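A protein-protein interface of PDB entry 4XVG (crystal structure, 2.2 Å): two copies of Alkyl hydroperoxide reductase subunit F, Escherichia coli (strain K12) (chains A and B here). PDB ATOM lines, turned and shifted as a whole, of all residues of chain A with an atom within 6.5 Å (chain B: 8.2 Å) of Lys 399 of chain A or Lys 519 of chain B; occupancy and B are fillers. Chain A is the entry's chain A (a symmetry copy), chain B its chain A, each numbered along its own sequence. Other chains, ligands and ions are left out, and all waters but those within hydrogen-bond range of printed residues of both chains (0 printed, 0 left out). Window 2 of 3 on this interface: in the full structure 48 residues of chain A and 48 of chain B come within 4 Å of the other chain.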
ATOM      1  N   ILE A 372      -5.963 -28.554 -12.613  1.00  0.00           N
ATOM      2  CA  ILE A 372      -7.276 -28.338 -11.986  1.00  0.00           C
ATOM      3  C   ILE A 372      -8.003 -27.180 -12.654  1.00  0.00           C
ATOM      4  O   ILE A 372      -9.194 -27.264 -12.948  1.00  0.00           O
ATOM      5  CB  ILE A 372      -7.132 -28.017 -10.475  1.00  0.00           C
ATOM      6  CG1 ILE A 372      -6.537 -29.224  -9.740  1.00  0.00           C
ATOM      7  CG2 ILE A 372      -8.482 -27.632  -9.857  1.00  0.00           C
ATOM      8  CD1 ILE A 372      -6.108 -28.926  -8.313  1.00  0.00           C
ATOM      9  N   GLN A 394      -0.386 -31.776  -1.024  1.00  0.00           N
ATOM     10  CA  GLN A 394      -1.295 -32.931  -1.039  1.00  0.00           C
ATOM     11  C   GLN A 394      -2.755 -32.560  -1.335  1.00  0.00           C
ATOM     12  O   GLN A 394      -3.463 -33.298  -2.020  1.00  0.00           O
ATOM     13  CB  GLN A 394      -1.218 -33.698   0.288  1.00  0.00           C
ATOM     14  CG  GLN A 394      -1.840 -35.097   0.229  1.00  0.00           C
ATOM     15  CD  GLN A 394      -1.026 -36.067  -0.632  1.00  0.00           C
ATOM     16  OE1 GLN A 394       0.199 -36.168  -0.486  1.00  0.00           O
ATOM     17  NE2 GLN A 394      -1.701 -36.776  -1.537  1.00  0.00           N
ATOM     18  N   VAL A 395      -3.197 -31.416  -0.819  1.00  0.00           N
ATOM     19  CA  VAL A 395      -4.572 -30.970  -1.032  1.00  0.00           C
ATOM     20  C   VAL A 395      -4.848 -30.767  -2.529  1.00  0.00           C
ATOM     21  O   VAL A 395      -5.923 -31.133  -3.030  1.00  0.00           O
ATOM     22  CB  VAL A 395      -4.906 -29.696  -0.181  1.00  0.00           C
ATOM     23  CG1 VAL A 395      -3.894 -28.580  -0.437  1.00  0.00           C
ATOM     24  CG2 VAL A 395      -6.315 -29.215  -0.447  1.00  0.00           C
ATOM     25  N   LEU A 396      -3.865 -30.215  -3.241  1.00  0.00           N
ATOM     26  CA  LEU A 396      -3.949 -30.071  -4.699  1.00  0.00           C
ATOM     27  C   LEU A 396      -3.999 -31.436  -5.409  1.00  0.00           C
ATOM     28  O   LEU A 396      -4.797 -31.634  -6.339  1.00  0.00           O
ATOM     29  CB  LEU A 396      -2.765 -29.254  -5.222  1.00  0.00           C
ATOM     30  CG  LEU A 396      -2.828 -27.730  -5.429  1.00  0.00           C
ATOM     31  CD1 LEU A 396      -4.054 -27.039  -4.821  1.00  0.00           C
ATOM     32  CD2 LEU A 396      -1.527 -27.082  -4.957  1.00  0.00           C
ATOM     33  N   GLN A 397      -3.158 -32.376  -4.971  1.00  0.00           N
ATOM     34  CA  GLN A 397      -3.124 -33.711  -5.579  1.00  0.00           C
ATOM     35  C   GLN A 397      -4.463 -34.399  -5.385  1.00  0.00           C
ATOM     36  O   GLN A 397      -5.002 -35.017  -6.315  1.00  0.00           O
ATOM     37  CB  GLN A 397      -2.024 -34.579  -4.945  1.00  0.00           C
ATOM     38  CG  GLN A 397      -0.592 -34.172  -5.255  1.00  0.00           C
ATOM     39  CD  GLN A 397       0.400 -35.281  -4.896  1.00  0.00           C
ATOM     40  OE1 GLN A 397       0.141 -36.464  -5.154  1.00  0.00           O
ATOM     41  NE2 GLN A 397       1.534 -34.905  -4.296  1.00  0.00           N
ATOM     42  N   ASP A 398      -4.989 -34.301  -4.165  1.00  0.00           N
ATOM     43  CA  ASP A 398      -6.296 -34.879  -3.846  1.00  0.00           C
ATOM     44  C   ASP A 398      -7.375 -34.260  -4.729  1.00  0.00           C
ATOM     45  O   ASP A 398      -8.188 -34.972  -5.314  1.00  0.00           O
ATOM     46  CB  ASP A 398      -6.646 -34.646  -2.375  1.00  0.00           C
ATOM     47  CG  ASP A 398      -5.826 -35.519  -1.423  1.00  0.00           C
ATOM     48  OD1 ASP A 398      -6.083 -35.453  -0.197  1.00  0.00           O
ATOM     49  OD2 ASP A 398      -4.938 -36.272  -1.893  1.00  0.00           O
ATOM     50  N   LYS A 399      -7.373 -32.934  -4.829  1.00  0.00           N
ATOM     51  CA  LYS A 399      -8.350 -32.246  -5.665  1.00  0.00           C
ATOM     52  C   LYS A 399      -8.270 -32.758  -7.106  1.00  0.00           C
ATOM     53  O   LYS A 399      -9.283 -33.175  -7.668  1.00  0.00           O
ATOM     54  CB  LYS A 399      -8.156 -30.727  -5.607  1.00  0.00           C
ATOM     55  CG  LYS A 399      -9.163 -29.939  -6.440  1.00  0.00           C
ATOM     56  CD  LYS A 399     -10.584 -30.152  -5.936  1.00  0.00           C
ATOM     57  CE  LYS A 399     -11.290 -28.818  -5.697  1.00  0.00           C
ATOM     58  NZ  LYS A 399     -12.394 -28.948  -4.692  1.00  0.00           N
ATOM     59  N   LEU A 400      -7.065 -32.781  -7.677  1.00  0.00           N
ATOM     60  CA  LEU A 400      -6.883 -33.215  -9.074  1.00  0.00           C
ATOM     61  C   LEU A 400      -7.372 -34.644  -9.329  1.00  0.00           C
ATOM     62  O   LEU A 400      -8.088 -34.888 -10.304  1.00  0.00           O
ATOM     63  CB  LEU A 400      -5.418 -33.058  -9.520  1.00  0.00           C
ATOM     64  CG  LEU A 400      -5.144 -33.347 -10.997  1.00  0.00           C
ATOM     65  CD1 LEU A 400      -6.009 -32.454 -11.875  1.00  0.00           C
ATOM     66  CD2 LEU A 400      -3.658 -33.176 -11.355  1.00  0.00           C
ATOM     67  N   ARG A 401      -7.005 -35.578  -8.449  1.00  0.00           N
ATOM     68  CA  ARG A 401      -7.466 -36.968  -8.552  1.00  0.00           C
ATOM     69  C   ARG A 401      -8.984 -37.132  -8.399  1.00  0.00           C
ATOM     70  O   ARG A 401      -9.544 -38.147  -8.808  1.00  0.00           O
ATOM     71  CB  ARG A 401      -6.736 -37.871  -7.534  1.00  0.00           C
ATOM     72  CG  ARG A 401      -5.225 -37.969  -7.754  1.00  0.00           C
ATOM     73  CD  ARG A 401      -4.603 -39.171  -7.045  1.00  0.00           C
ATOM     74  NE  ARG A 401      -3.184 -39.321  -7.391  1.00  0.00           N
ATOM     75  CZ  ARG A 401      -2.729 -40.025  -8.430  1.00  0.00           C
ATOM     76  NH1 ARG A 401      -3.571 -40.671  -9.235  1.00  0.00           N
ATOM     77  NH2 ARG A 401      -1.423 -40.095  -8.665  1.00  0.00           N
ATOM     78  N   SER A 402      -9.641 -36.146  -7.794  1.00  0.00           N
ATOM     79  CA  SER A 402     -11.097 -36.183  -7.651  1.00  0.00           C
ATOM     80  C   SER A 402     -11.798 -35.828  -8.960  1.00  0.00           C
ATOM     81  O   SER A 402     -13.017 -35.998  -9.089  1.00  0.00           O
ATOM     82  CB  SER A 402     -11.548 -35.195  -6.571  1.00  0.00           C
ATOM     83  OG  SER A 402     -11.492 -33.867  -7.063  1.00  0.00           O
ATOM     84  N   LEU A 403     -11.039 -35.331  -9.933  1.00  0.00           N
ATOM     85  CA  LEU A 403     -11.651 -34.833 -11.167  1.00  0.00           C
ATOM     86  C   LEU A 403     -11.900 -35.950 -12.185  1.00  0.00           C
ATOM     87  O   LEU A 403     -11.114 -36.896 -12.304  1.00  0.00           O
ATOM     88  CB  LEU A 403     -10.826 -33.680 -11.763  1.00  0.00           C
ATOM     89  CG  LEU A 403     -10.769 -32.433 -10.868  1.00  0.00           C
ATOM     90  CD1 LEU A 403      -9.970 -31.287 -11.501  1.00  0.00           C
ATOM     91  CD2 LEU A 403     -12.176 -31.970 -10.520  1.00  0.00           C
ATOM     92  N   ALA B 212     -25.744 -18.540  -5.214  1.00  0.00           N
ATOM     93  CA  ALA B 212     -24.447 -18.229  -4.623  1.00  0.00           C
ATOM     94  C   ALA B 212     -23.371 -18.126  -5.701  1.00  0.00           C
ATOM     95  O   ALA B 212     -23.447 -18.780  -6.750  1.00  0.00           O
ATOM     96  CB  ALA B 212     -24.065 -19.265  -3.604  1.00  0.00           C
ATOM     97  N   TYR B 213     -22.371 -17.296  -5.448  1.00  0.00           N
ATOM     98  CA  TYR B 213     -21.320 -17.075  -6.426  1.00  0.00           C
ATOM     99  C   TYR B 213     -20.073 -17.837  -6.026  1.00  0.00           C
ATOM    100  O   TYR B 213     -19.878 -18.155  -4.843  1.00  0.00           O
ATOM    101  CB  TYR B 213     -21.006 -15.576  -6.538  1.00  0.00           C
ATOM    102  CG  TYR B 213     -22.125 -14.752  -7.130  1.00  0.00           C
ATOM    103  CD1 TYR B 213     -23.063 -14.130  -6.312  1.00  0.00           C
ATOM    104  CD2 TYR B 213     -22.239 -14.584  -8.505  1.00  0.00           C
ATOM    105  CE1 TYR B 213     -24.098 -13.377  -6.851  1.00  0.00           C
ATOM    106  CE2 TYR B 213     -23.265 -13.822  -9.052  1.00  0.00           C
ATOM    107  CZ  TYR B 213     -24.190 -13.223  -8.218  1.00  0.00           C
ATOM    108  OH  TYR B 213     -25.212 -12.467  -8.746  1.00  0.00           O
ATOM    109  N   ASP B 214     -19.226 -18.139  -7.009  1.00  0.00           N
ATOM    110  CA  ASP B 214     -17.905 -18.685  -6.709  1.00  0.00           C
ATOM    111  C   ASP B 214     -17.064 -17.553  -6.139  1.00  0.00           C
ATOM    112  O   ASP B 214     -16.380 -17.703  -5.117  1.00  0.00           O
ATOM    113  CB  ASP B 214     -17.271 -19.250  -7.974  1.00  0.00           C
ATOM    114  CG  ASP B 214     -17.815 -20.623  -8.320  1.00  0.00           C
ATOM    115  OD1 ASP B 214     -17.910 -21.468  -7.401  1.00  0.00           O
ATOM    116  OD2 ASP B 214     -18.176 -20.857  -9.485  1.00  0.00           O
ATOM    117  N   VAL B 215     -17.149 -16.406  -6.804  1.00  0.00           N
ATOM    118  CA  VAL B 215     -16.492 -15.199  -6.343  1.00  0.00           C
ATOM    119  C   VAL B 215     -17.438 -14.026  -6.534  1.00  0.00           C
ATOM    120  O   VAL B 215     -18.092 -13.895  -7.582  1.00  0.00           O
ATOM    121  CB  VAL B 215     -15.151 -14.940  -7.077  1.00  0.00           C
ATOM    122  CG1 VAL B 215     -15.376 -14.761  -8.574  1.00  0.00           C
ATOM    123  CG2 VAL B 215     -14.463 -13.707  -6.492  1.00  0.00           C
ATOM    124  N   ILE B 236     -15.547 -19.758 -13.703  1.00  0.00           N
ATOM    125  CA  ILE B 236     -16.291 -19.799 -12.447  1.00  0.00           C
ATOM    126  C   ILE B 236     -17.430 -18.776 -12.414  1.00  0.00           C
ATOM    127  O   ILE B 236     -17.400 -17.768 -13.126  1.00  0.00           O
ATOM    128  CB  ILE B 236     -15.383 -19.572 -11.212  1.00  0.00           C
ATOM    129  CG1 ILE B 236     -14.885 -18.126 -11.173  1.00  0.00           C
ATOM    130  CG2 ILE B 236     -14.246 -20.608 -11.172  1.00  0.00           C
ATOM    131  CD1 ILE B 236     -13.899 -17.845 -10.035  1.00  0.00           C
ATOM    132  N   ARG B 237     -18.424 -19.045 -11.566  1.00  0.00           N
ATOM    133  CA  ARG B 237     -19.562 -18.148 -11.379  1.00  0.00           C
ATOM    134  C   ARG B 237     -19.119 -16.833 -10.723  1.00  0.00           C
ATOM    135  O   ARG B 237     -18.864 -16.765  -9.507  1.00  0.00           O
ATOM    136  CB  ARG B 237     -20.662 -18.834 -10.551  1.00  0.00           C
ATOM    137  CG  ARG B 237     -21.861 -17.919 -10.240  1.00  0.00           C
ATOM    138  CD  ARG B 237     -23.175 -18.689 -10.015  1.00  0.00           C
ATOM    139  NE  ARG B 237     -24.147 -17.836  -9.324  1.00  0.00           N
ATOM    140  CZ  ARG B 237     -24.951 -16.960  -9.923  1.00  0.00           C
ATOM    141  NH1 ARG B 237     -24.924 -16.815 -11.247  1.00  0.00           N
ATOM    142  NH2 ARG B 237     -25.784 -16.222  -9.195  1.00  0.00           N
ATOM    143  N   GLU B 299     -14.252 -21.962   7.627  1.00  0.00           N
ATOM    144  CA  GLU B 299     -13.593 -21.940   6.323  1.00  0.00           C
ATOM    145  C   GLU B 299     -14.241 -22.958   5.395  1.00  0.00           C
ATOM    146  O   GLU B 299     -14.443 -24.110   5.782  1.00  0.00           O
ATOM    147  CB  GLU B 299     -12.105 -22.265   6.471  1.00  0.00           C
ATOM    148  CG  GLU B 299     -11.290 -22.016   5.205  1.00  0.00           C
ATOM    149  CD  GLU B 299      -9.932 -22.691   5.241  1.00  0.00           C
ATOM    150  OE1 GLU B 299      -8.915 -22.016   4.963  1.00  0.00           O
ATOM    151  OE2 GLU B 299      -9.886 -23.908   5.529  1.00  0.00           O
ATOM    152  N   GLY B 300     -14.566 -22.537   4.173  1.00  0.00           N
ATOM    153  CA  GLY B 300     -15.271 -23.393   3.231  1.00  0.00           C
ATOM    154  C   GLY B 300     -16.745 -23.031   3.098  1.00  0.00           C
ATOM    155  O   GLY B 300     -17.391 -23.369   2.100  1.00  0.00           O
ATOM    156  N   LEU B 302     -20.120 -20.247   3.109  1.00  0.00           N
ATOM    157  CA  LEU B 302     -20.476 -19.122   2.247  1.00  0.00           C
ATOM    158  C   LEU B 302     -20.337 -17.789   2.979  1.00  0.00           C
ATOM    159  O   LEU B 302     -20.802 -17.634   4.108  1.00  0.00           O
ATOM    160  CB  LEU B 302     -21.914 -19.261   1.741  1.00  0.00           C
ATOM    161  CG  LEU B 302     -22.211 -20.419   0.781  1.00  0.00           C
ATOM    162  CD1 LEU B 302     -23.673 -20.383   0.374  1.00  0.00           C
ATOM    163  CD2 LEU B 302     -21.345 -20.309  -0.455  1.00  0.00           C
ATOM    164  N   ARG B 316     -18.715 -18.110  -2.282  1.00  0.00           N
ATOM    165  CA  ARG B 316     -17.647 -18.935  -1.739  1.00  0.00           C
ATOM    166  C   ARG B 316     -16.395 -18.095  -1.441  1.00  0.00           C
ATOM    167  O   ARG B 316     -15.612 -18.415  -0.534  1.00  0.00           O
ATOM    168  CB  ARG B 316     -17.325 -20.065  -2.735  1.00  0.00           C
ATOM    169  CG  ARG B 316     -17.819 -21.471  -2.335  1.00  0.00           C
ATOM    170  CD  ARG B 316     -19.239 -21.789  -2.805  1.00  0.00           C
ATOM    171  NE  ARG B 316     -19.428 -21.801  -4.263  1.00  0.00           N
ATOM    172  CZ  ARG B 316     -20.536 -22.244  -4.876  1.00  0.00           C
ATOM    173  NH1 ARG B 316     -21.550 -22.733  -4.160  1.00  0.00           N
ATOM    174  NH2 ARG B 316     -20.638 -22.209  -6.206  1.00  0.00           N
ATOM    175  N   SER B 317     -16.195 -17.022  -2.206  1.00  0.00           N
ATOM    176  CA  SER B 317     -15.069 -16.120  -1.947  1.00  0.00           C
ATOM    177  C   SER B 317     -15.472 -14.690  -2.246  1.00  0.00           C
ATOM    178  O   SER B 317     -16.358 -14.444  -3.084  1.00  0.00           O
ATOM    179  CB  SER B 317     -13.857 -16.506  -2.806  1.00  0.00           C
ATOM    180  OG  SER B 317     -14.157 -16.379  -4.193  1.00  0.00           O
ATOM    181  N   ALA B 511      -8.006 -15.684  -5.078  1.00  0.00           N
ATOM    182  CA  ALA B 511      -9.333 -16.196  -4.754  1.00  0.00           C
ATOM    183  C   ALA B 511      -9.562 -17.529  -5.446  1.00  0.00           C
ATOM    184  O   ALA B 511     -10.183 -18.422  -4.876  1.00  0.00           O
ATOM    185  CB  ALA B 511     -10.412 -15.187  -5.148  1.00  0.00           C
ATOM    186  N   PHE B 512      -9.055 -17.664  -6.672  1.00  0.00           N
ATOM    187  CA  PHE B 512      -9.204 -18.906  -7.400  1.00  0.00           C
ATOM    188  C   PHE B 512      -8.403 -20.037  -6.742  1.00  0.00           C
ATOM    189  O   PHE B 512      -8.912 -21.151  -6.565  1.00  0.00           O
ATOM    190  CB  PHE B 512      -8.781 -18.751  -8.862  1.00  0.00           C
ATOM    191  CG  PHE B 512      -9.041 -19.974  -9.675  1.00  0.00           C
ATOM    192  CD1 PHE B 512     -10.347 -20.403  -9.893  1.00  0.00           C
ATOM    193  CD2 PHE B 512      -7.997 -20.722 -10.186  1.00  0.00           C
ATOM    194  CE1 PHE B 512     -10.610 -21.541 -10.624  1.00  0.00           C
ATOM    195  CE2 PHE B 512      -8.253 -21.864 -10.929  1.00  0.00           C
ATOM    196  CZ  PHE B 512      -9.561 -22.280 -11.139  1.00  0.00           C
ATOM    197  N   ASP B 513      -7.143 -19.753  -6.409  1.00  0.00           N
ATOM    198  CA  ASP B 513      -6.331 -20.690  -5.642  1.00  0.00           C
ATOM    199  C   ASP B 513      -7.020 -21.108  -4.344  1.00  0.00           C
ATOM    200  O   ASP B 513      -6.966 -22.276  -3.954  1.00  0.00           O
ATOM    201  CB  ASP B 513      -4.969 -20.086  -5.310  1.00  0.00           C
ATOM    202  CG  ASP B 513      -4.164 -20.970  -4.372  1.00  0.00           C
ATOM    203  OD1 ASP B 513      -4.057 -20.651  -3.163  1.00  0.00           O
ATOM    204  OD2 ASP B 513      -3.651 -22.007  -4.839  1.00  0.00           O
ATOM    205  N   TYR B 514      -7.674 -20.161  -3.676  1.00  0.00           N
ATOM    206  CA  TYR B 514      -8.417 -20.489  -2.466  1.00  0.00           C
ATOM    207  C   TYR B 514      -9.579 -21.451  -2.745  1.00  0.00           C
ATOM    208  O   TYR B 514      -9.834 -22.353  -1.948  1.00  0.00           O
ATOM    209  CB  TYR B 514      -8.949 -19.213  -1.797  1.00  0.00           C
ATOM    210  CG  TYR B 514      -9.931 -19.492  -0.672  1.00  0.00           C
ATOM    211  CD1 TYR B 514      -9.488 -19.703   0.630  1.00  0.00           C
ATOM    212  CD2 TYR B 514     -11.295 -19.544  -0.919  1.00  0.00           C
ATOM    213  CE1 TYR B 514     -10.386 -19.953   1.659  1.00  0.00           C
ATOM    214  CE2 TYR B 514     -12.201 -19.796   0.097  1.00  0.00           C
ATOM    215  CZ  TYR B 514     -11.744 -19.994   1.384  1.00  0.00           C
ATOM    216  OH  TYR B 514     -12.660 -20.241   2.394  1.00  0.00           O
ATOM    217  N   LEU B 515     -10.300 -21.243  -3.851  1.00  0.00           N
ATOM    218  CA  LEU B 515     -11.415 -22.129  -4.220  1.00  0.00           C
ATOM    219  C   LEU B 515     -10.931 -23.541  -4.544  1.00  0.00           C
ATOM    220  O   LEU B 515     -11.624 -24.538  -4.294  1.00  0.00           O
ATOM    221  CB  LEU B 515     -12.167 -21.592  -5.437  1.00  0.00           C
ATOM    222  CG  LEU B 515     -13.025 -20.332  -5.258  1.00  0.00           C
ATOM    223  CD1 LEU B 515     -13.559 -19.888  -6.608  1.00  0.00           C
ATOM    224  CD2 LEU B 515     -14.178 -20.606  -4.298  1.00  0.00           C
ATOM    225  N   ILE B 516      -9.747 -23.634  -5.128  1.00  0.00           N
ATOM    226  CA  ILE B 516      -9.225 -24.950  -5.483  1.00  0.00           C
ATOM    227  C   ILE B 516      -8.918 -25.745  -4.214  1.00  0.00           C
ATOM    228  O   ILE B 516      -9.185 -26.951  -4.140  1.00  0.00           O
ATOM    229  CB  ILE B 516      -7.983 -24.830  -6.390  1.00  0.00           C
ATOM    230  CG1 ILE B 516      -8.419 -24.413  -7.808  1.00  0.00           C
ATOM    231  CG2 ILE B 516      -7.242 -26.134  -6.461  1.00  0.00           C
ATOM    232  CD1 ILE B 516      -7.242 -24.239  -8.760  1.00  0.00           C
ATOM    233  N   ARG B 517      -8.408 -25.055  -3.196  1.00  0.00           N
ATOM    234  CA  ARG B 517      -7.954 -25.713  -1.968  1.00  0.00           C
ATOM    235  C   ARG B 517      -9.053 -26.012  -0.946  1.00  0.00           C
ATOM    236  O   ARG B 517      -8.832 -26.810  -0.034  1.00  0.00           O
ATOM    237  CB  ARG B 517      -6.838 -24.890  -1.310  1.00  0.00           C
ATOM    238  CG  ARG B 517      -5.563 -24.798  -2.149  1.00  0.00           C
ATOM    239  CD  ARG B 517      -4.582 -23.814  -1.521  1.00  0.00           C
ATOM    240  NE  ARG B 517      -3.349 -23.687  -2.296  1.00  0.00           N
ATOM    241  CZ  ARG B 517      -2.290 -24.487  -2.159  1.00  0.00           C
ATOM    242  NH1 ARG B 517      -2.306 -25.478  -1.274  1.00  0.00           N
ATOM    243  NH2 ARG B 517      -1.209 -24.295  -2.906  1.00  0.00           N
ATOM    244  N   THR B 518     -10.223 -25.387  -1.092  1.00  0.00           N
ATOM    245  CA  THR B 518     -11.288 -25.529  -0.086  1.00  0.00           C
ATOM    246  C   THR B 518     -12.608 -26.129  -0.596  1.00  0.00           C
ATOM    247  O   THR B 518     -13.368 -26.704   0.190  1.00  0.00           O
ATOM    248  CB  THR B 518     -11.598 -24.187   0.634  1.00  0.00           C
ATOM    249  OG1 THR B 518     -12.160 -23.254  -0.305  1.00  0.00           O
ATOM    250  CG2 THR B 518     -10.331 -23.593   1.271  1.00  0.00           C
ATOM    251  N   LYS B 519     -12.880 -25.993  -1.894  1.00  0.00           N
ATOM    252  CA  LYS B 519     -14.139 -26.489  -2.483  1.00  0.00           C
ATOM    253  C   LYS B 519     -14.286 -28.014  -2.459  1.00  0.00           C
ATOM    254  O   LYS B 519     -15.385 -28.549  -2.651  1.00  0.00           O
ATOM    255  CB  LYS B 519     -14.320 -25.979  -3.919  1.00  0.00           C
ATOM    256  CG  LYS B 519     -15.131 -24.690  -4.035  1.00  0.00           C
ATOM    257  CD  LYS B 519     -16.391 -24.929  -4.858  1.00  0.00           C
ATOM    258  CE  LYS B 519     -16.602 -23.824  -5.875  1.00  0.00           C
ATOM    259  NZ  LYS B 519     -17.504 -24.270  -6.991  1.00  0.00           N
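Printed residues of chain B within 4 Å of Ile 372 of chain A: Ile 516 (3.5 Å).
Of the printed residues of chain B, Val 395 of chain A touches Arg 517 (3.5 Å).
Of the printed residues of chain B, Leu 396 of chain A touches Ile 516 (3.7 Å) and Arg 517 (3.5 Å).
Lys 399 of chain A touches just these residues of chain B: Ile 516 and Lys 519.
Ala 212 of chain B touches none of the printed residues of chain A.
Tyr 213 of chain B touches none of the printed residues of chain A.
Printed residues of chain A within 4 Å of Ile 516 of chain B: Ile 372 (3.5 Å), Leu 396 (3.7 Å) and Lys 399 (3.2 Å).
Of the printed residues of chain A, Arg 517 of chain B touches Val 395 (3.5 Å) and Leu 396 (3.5 Å).
Of chain A, only Lys 399 comes within 4 Å of Lys 519 of chain B.
Among the printed residues, pairs that only touch across the chains: Ile 372 of chain A with Ile 516 of chain B (3.5 Å), Val 395 of chain A with Arg 517 of chain B (3.5 Å), Leu 396 of chain A with Ile 516 of chain B (3.7 Å), Leu 396 of chain A with Arg 517 of chain B (3.5 Å), Lys 399 of chain A with Ile 516 of chain B (3.2 Å) and Lys 399 of chain A with Lys 519 of chain B (3.1 Å).
The side-chain carboxylate (OD1) of Asp 214 of chain B lies within salt-bridge range of the side-chain amino group (NZ) of Lys 519 of chain B, at 2.9 Å.
NE of Arg 517 of chain B lies within salt-bridge range of OD2 of Asp 513 of chain B (3.1 Å).
No position is printed for both chains.
Of the 6 pairs that touch across the chains among the printed residues, none has its exchanged pair printed and touching as well.
Hydrophobic or aromatic side chains of chain B within 4 Å of the printed part of chain A: Ile 516.
Hydrophobic or aromatic side chains of chain A within 4 Å of the printed part of chain B: Ile 372, Val 395 and Leu 396.
Among the printed residues, no Asp or Glu carboxylate lies within 4 Å of a Lys or Arg side-chain nitrogen of the other chain.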
